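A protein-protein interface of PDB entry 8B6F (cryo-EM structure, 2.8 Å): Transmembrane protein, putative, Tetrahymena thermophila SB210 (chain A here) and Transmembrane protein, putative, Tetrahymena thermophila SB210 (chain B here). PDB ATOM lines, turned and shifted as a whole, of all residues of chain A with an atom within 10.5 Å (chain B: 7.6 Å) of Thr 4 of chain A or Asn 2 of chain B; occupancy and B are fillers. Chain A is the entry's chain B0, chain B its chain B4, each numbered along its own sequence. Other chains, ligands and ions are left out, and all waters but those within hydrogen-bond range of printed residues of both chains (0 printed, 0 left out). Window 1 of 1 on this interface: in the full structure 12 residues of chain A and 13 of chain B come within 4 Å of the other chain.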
ATOM      1  N   VAL A   2      12.605  12.464   3.098  1.00  0.00           N
ATOM      2  CA  VAL A   2      13.893  13.175   2.872  1.00  0.00           C
ATOM      3  C   VAL A   2      14.429  13.725   4.186  1.00  0.00           C
ATOM      4  O   VAL A   2      14.307  14.915   4.472  1.00  0.00           O
ATOM      5  CB  VAL A   2      13.735  14.304   1.835  1.00  0.00           C
ATOM      6  CG1 VAL A   2      13.674  13.725   0.432  1.00  0.00           C
ATOM      7  CG2 VAL A   2      12.491  15.138   2.124  1.00  0.00           C
ATOM      8  N   ASN A   3      15.024  12.846   4.987  1.00  0.00           N
ATOM      9  CA  ASN A   3      15.622  13.230   6.264  1.00  0.00           C
ATOM     10  C   ASN A   3      17.036  13.724   5.992  1.00  0.00           C
ATOM     11  O   ASN A   3      17.995  12.953   5.965  1.00  0.00           O
ATOM     12  CB  ASN A   3      15.611  12.057   7.235  1.00  0.00           C
ATOM     13  CG  ASN A   3      16.304  12.378   8.541  1.00  0.00           C
ATOM     14  OD1 ASN A   3      16.473  13.543   8.897  1.00  0.00           O
ATOM     15  ND2 ASN A   3      16.706  11.342   9.268  1.00  0.00           N
ATOM     16  N   THR A   4      17.165  15.033   5.783  1.00  0.00           N
ATOM     17  CA  THR A   4      18.462  15.649   5.504  1.00  0.00           C
ATOM     18  C   THR A   4      19.176  16.005   6.809  1.00  0.00           C
ATOM     19  O   THR A   4      19.533  17.152   7.072  1.00  0.00           O
ATOM     20  CB  THR A   4      18.284  16.877   4.618  1.00  0.00           C
ATOM     21  OG1 THR A   4      17.468  17.846   5.290  1.00  0.00           O
ATOM     22  CG2 THR A   4      17.631  16.494   3.297  1.00  0.00           C
ATOM     23  N   ALA A   5      19.377  14.983   7.634  1.00  0.00           N
ATOM     24  CA  ALA A   5      20.050  15.164   8.908  1.00  0.00           C
ATOM     25  C   ALA A   5      21.565  15.174   8.718  1.00  0.00           C
ATOM     26  O   ALA A   5      22.094  14.785   7.674  1.00  0.00           O
ATOM     27  CB  ALA A   5      19.643  14.061   9.884  1.00  0.00           C
ATOM     28  N   TYR A   6      22.266  15.633   9.751  1.00  0.00           N
ATOM     29  CA  TYR A   6      23.717  15.655   9.711  1.00  0.00           C
ATOM     30  C   TYR A   6      24.268  14.229   9.703  1.00  0.00           C
ATOM     31  O   TYR A   6      23.617  13.302  10.189  1.00  0.00           O
ATOM     32  CB  TYR A   6      24.279  16.401  10.918  1.00  0.00           C
ATOM     33  CG  TYR A   6      24.102  17.900  10.878  1.00  0.00           C
ATOM     34  CD1 TYR A   6      22.852  18.478  11.031  1.00  0.00           C
ATOM     35  CD2 TYR A   6      25.197  18.738  10.729  1.00  0.00           C
ATOM     36  CE1 TYR A   6      22.692  19.850  11.011  1.00  0.00           C
ATOM     37  CE2 TYR A   6      25.049  20.109  10.708  1.00  0.00           C
ATOM     38  CZ  TYR A   6      23.794  20.659  10.850  1.00  0.00           C
ATOM     39  OH  TYR A   6      23.643  22.025  10.831  1.00  0.00           O
ATOM     40  N   PRO A   7      25.461  14.027   9.149  1.00  0.00           N
ATOM     41  CA  PRO A   7      26.141  12.744   9.343  1.00  0.00           C
ATOM     42  C   PRO A   7      26.408  12.489  10.818  1.00  0.00           C
ATOM     43  O   PRO A   7      26.626  13.413  11.603  1.00  0.00           O
ATOM     44  CB  PRO A   7      27.447  12.909   8.556  1.00  0.00           C
ATOM     45  CG  PRO A   7      27.155  13.957   7.553  1.00  0.00           C
ATOM     46  CD  PRO A   7      26.183  14.894   8.204  1.00  0.00           C
ATOM     47  N   THR A   8      26.382  11.213  11.189  1.00  0.00           N
ATOM     48  CA  THR A   8      26.601  10.843  12.586  1.00  0.00           C
ATOM     49  C   THR A   8      27.926  11.355  13.131  1.00  0.00           C
ATOM     50  O   THR A   8      27.931  11.941  14.227  1.00  0.00           O
ATOM     51  CB  THR A   8      26.494   9.322  12.731  1.00  0.00           C
ATOM     52  OG1 THR A   8      25.115   8.934  12.719  1.00  0.00           O
ATOM     53  CG2 THR A   8      27.148   8.849  14.022  1.00  0.00           C
ATOM     54  N   LEU A  10      29.788  13.950  12.273  1.00  0.00           N
ATOM     55  CA  LEU A  10      29.742  15.400  12.422  1.00  0.00           C
ATOM     56  C   LEU A  10      28.815  15.809  13.560  1.00  0.00           C
ATOM     57  O   LEU A  10      29.145  16.706  14.343  1.00  0.00           O
ATOM     58  CB  LEU A  10      29.304  16.051  11.110  1.00  0.00           C
ATOM     59  CG  LEU A  10      29.368  17.580  11.072  1.00  0.00           C
ATOM     60  CD1 LEU A  10      30.789  18.075  11.281  1.00  0.00           C
ATOM     61  CD2 LEU A  10      28.815  18.097   9.759  1.00  0.00           C
ATOM     62  N   LYS A  11      27.660  15.153  13.681  1.00  0.00           N
ATOM     63  CA  LYS A  11      26.734  15.482  14.760  1.00  0.00           C
ATOM     64  C   LYS A  11      27.358  15.207  16.123  1.00  0.00           C
ATOM     65  O   LYS A  11      27.175  15.985  17.067  1.00  0.00           O
ATOM     66  CB  LYS A  11      25.436  14.693  14.600  1.00  0.00           C
ATOM     67  CG  LYS A  11      24.245  15.355  15.268  1.00  0.00           C
ATOM     68  CD  LYS A  11      23.040  14.437  15.329  1.00  0.00           C
ATOM     69  CE  LYS A  11      23.201  13.393  16.420  1.00  0.00           C
ATOM     70  NZ  LYS A  11      21.965  12.581  16.595  1.00  0.00           N
ATOM     71  N   MET B   1      11.485  22.634   0.268  1.00  0.00           N
ATOM     72  CA  MET B   1      11.562  23.537   1.449  1.00  0.00           C
ATOM     73  C   MET B   1      12.789  23.211   2.292  1.00  0.00           C
ATOM     74  O   MET B   1      13.380  24.093   2.914  1.00  0.00           O
ATOM     75  CB  MET B   1      10.292  23.421   2.296  1.00  0.00           C
ATOM     76  CG  MET B   1      10.262  24.360   3.493  1.00  0.00           C
ATOM     77  SD  MET B   1       8.720  24.268   4.421  1.00  0.00           S
ATOM     78  CE  MET B   1       9.037  25.463   5.716  1.00  0.00           C
ATOM     79  N   ASN B   2      13.170  21.938   2.304  1.00  0.00           N
ATOM     80  CA  ASN B   2      14.310  21.501   3.093  1.00  0.00           C
ATOM     81  C   ASN B   2      15.609  22.046   2.507  1.00  0.00           C
ATOM     82  O   ASN B   2      15.687  22.428   1.335  1.00  0.00           O
ATOM     83  CB  ASN B   2      14.368  19.976   3.157  1.00  0.00           C
ATOM     84  CG  ASN B   2      14.501  19.340   1.789  1.00  0.00           C
ATOM     85  OD1 ASN B   2      14.017  19.877   0.793  1.00  0.00           O
ATOM     86  ND2 ASN B   2      15.163  18.190   1.734  1.00  0.00           N
ATOM     87  N   LEU B   3      16.639  22.076   3.345  1.00  0.00           N
ATOM     88  CA  LEU B   3      17.966  22.524   2.964  1.00  0.00           C
ATOM     89  C   LEU B   3      18.985  21.450   3.312  1.00  0.00           C
ATOM     90  O   LEU B   3      18.779  20.676   4.253  1.00  0.00           O
ATOM     91  CB  LEU B   3      18.340  23.834   3.675  1.00  0.00           C
ATOM     92  CG  LEU B   3      17.529  25.079   3.299  1.00  0.00           C
ATOM     93  CD1 LEU B   3      17.913  26.256   4.180  1.00  0.00           C
ATOM     94  CD2 LEU B   3      17.721  25.434   1.834  1.00  0.00           C
ATOM     95  N   PRO B   4      20.089  21.374   2.570  1.00  0.00           N
ATOM     96  CA  PRO B   4      21.100  20.351   2.863  1.00  0.00           C
ATOM     97  C   PRO B   4      21.745  20.563   4.223  1.00  0.00           C
ATOM     98  O   PRO B   4      21.886  21.688   4.704  1.00  0.00           O
ATOM     99  CB  PRO B   4      22.121  20.521   1.731  1.00  0.00           C
ATOM    100  CG  PRO B   4      21.400  21.238   0.657  1.00  0.00           C
ATOM    101  CD  PRO B   4      20.407  22.120   1.341  1.00  0.00           C
ATOM    102  N   TRP B   5      22.136  19.450   4.844  1.00  0.00           N
ATOM    103  CA  TRP B   5      22.831  19.518   6.124  1.00  0.00           C
ATOM    104  C   TRP B   5      24.115  20.328   6.009  1.00  0.00           C
ATOM    105  O   TRP B   5      24.461  21.089   6.919  1.00  0.00           O
ATOM    106  CB  TRP B   5      23.135  18.109   6.635  1.00  0.00           C
ATOM    107  CG  TRP B   5      24.160  17.379   5.819  1.00  0.00           C
ATOM    108  CD1 TRP B   5      23.922  16.488   4.817  1.00  0.00           C
ATOM    109  CD2 TRP B   5      25.586  17.479   5.939  1.00  0.00           C
ATOM    110  NE1 TRP B   5      25.109  16.025   4.304  1.00  0.00           N
ATOM    111  CE2 TRP B   5      26.145  16.619   4.976  1.00  0.00           C
ATOM    112  CE3 TRP B   5      26.442  18.215   6.766  1.00  0.00           C
ATOM    113  CZ2 TRP B   5      27.522  16.473   4.816  1.00  0.00           C
ATOM    114  CZ3 TRP B   5      27.808  18.068   6.606  1.00  0.00           C
ATOM    115  CH2 TRP B   5      28.335  17.203   5.638  1.00  0.00           C
ATOM    116  N   PHE B   6      24.839  20.177   4.898  1.00  0.00           N
ATOM    117  CA  PHE B   6      26.070  20.939   4.724  1.00  0.00           C
ATOM    118  C   PHE B   6      25.781  22.420   4.518  1.00  0.00           C
ATOM    119  O   PHE B   6      26.593  23.264   4.912  1.00  0.00           O
ATOM    120  CB  PHE B   6      26.892  20.374   3.563  1.00  0.00           C
ATOM    121  CG  PHE B   6      26.134  20.250   2.271  1.00  0.00           C
ATOM    122  CD1 PHE B   6      25.988  21.338   1.430  1.00  0.00           C
ATOM    123  CD2 PHE B   6      25.596  19.032   1.886  1.00  0.00           C
ATOM    124  CE1 PHE B   6      25.304  21.220   0.235  1.00  0.00           C
ATOM    125  CE2 PHE B   6      24.911  18.907   0.694  1.00  0.00           C
ATOM    126  CZ  PHE B   6      24.765  20.002  -0.133  1.00  0.00           C
ATOM    127  N   ARG B   8      23.305  24.021   6.037  1.00  0.00           N
ATOM    128  CA  ARG B   8      23.055  24.508   7.391  1.00  0.00           C
ATOM    129  C   ARG B   8      24.348  24.607   8.190  1.00  0.00           C
ATOM    130  O   ARG B   8      24.550  25.567   8.940  1.00  0.00           O
ATOM    131  CB  ARG B   8      22.050  23.599   8.097  1.00  0.00           C
ATOM    132  CG  ARG B   8      20.633  23.724   7.556  1.00  0.00           C
ATOM    133  CD  ARG B   8      19.917  22.387   7.561  1.00  0.00           C
ATOM    134  NE  ARG B   8      19.905  21.774   8.883  1.00  0.00           N
ATOM    135  CZ  ARG B   8      19.495  20.538   9.131  1.00  0.00           C
ATOM    136  NH1 ARG B   8      19.054  19.749   8.166  1.00  0.00           N
ATOM    137  NH2 ARG B   8      19.533  20.080  10.379  1.00  0.00           N
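OG1 of Thr 4 of chain A sits at hydrogen-bond distance from O of Leu 3 of chain B.
O of Thr 4 of chain A sits at hydrogen-bond distance from NH1 of Arg 8 of chain B (2.9 Å).
The side-chain amide oxygen (OD1) of Asn 3 of chain A lies close to the backbone NH (N) of Ala 5 of chain A (3.5 Å).
Among the printed residues, merely in contact across the chains: Tyr 6 of chain A with Arg 8 of chain B (3.2 Å), Leu 10 of chain A with Trp 5 of chain B (3.3 Å), Thr 4 of chain A with Asn 2 of chain B (3.4 Å), Pro 7 of chain A with Trp 5 of chain B (3.5 Å), Ala 5 of chain A with Trp 5 of chain B (3.6 Å), Thr 4 of chain A with Trp 5 of chain B (3.8 Å) and Tyr 6 of chain A with Trp 5 of chain B (3.96 Å).
Thr 4 of chain A touches four residues of chain B.
No residue of chain A comes within 4 Å of Met 1 of chain B.
No residue of chain A comes within 4 Å of Pro 4 of chain B.
Of the printed residues of chain B, Pro 7 of chain A touches Trp 5.
Of the printed residues of chain B, Tyr 6 of chain A touches Trp 5 (3.96 Å) and Arg 8 (3.2 Å).
Of the printed residues of chain A, Arg 8 of chain B touches Thr 4 and Tyr 6.
Of the printed residues of chain B, Leu 10 of chain A touches Trp 5.
The nearest residue of chain B that does not touch Thr 4 of chain A is Pro 4 of chain B (4.8 Å).
The nearest residue of chain A that does not touch Asn 2 of chain B is Val 2 of chain A (4.1 Å).
The nearest printed residue of chain A that does not touch Trp 5 of chain B is Asn 3 of chain A (7.0 Å).
Of the 9 printed residues of chain A, 5 touch a printed residue of chain B.
Hydrophobic or aromatic side chains of chain A within 4 Å of the printed part of chain B: Tyr 6, Pro 7 and Leu 10.
Of the 7 printed residues of chain B, 4 touch a printed residue of chain A.
Hydrophobic or aromatic side chains of chain B that line the printed part of chain A: Trp 5.
Among the printed residues, 9 pairs touch across the chains.
Among the printed residues, no Asp or Glu carboxylate lies within 4 Å of a Lys or Arg side-chain nitrogen of the other chain.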
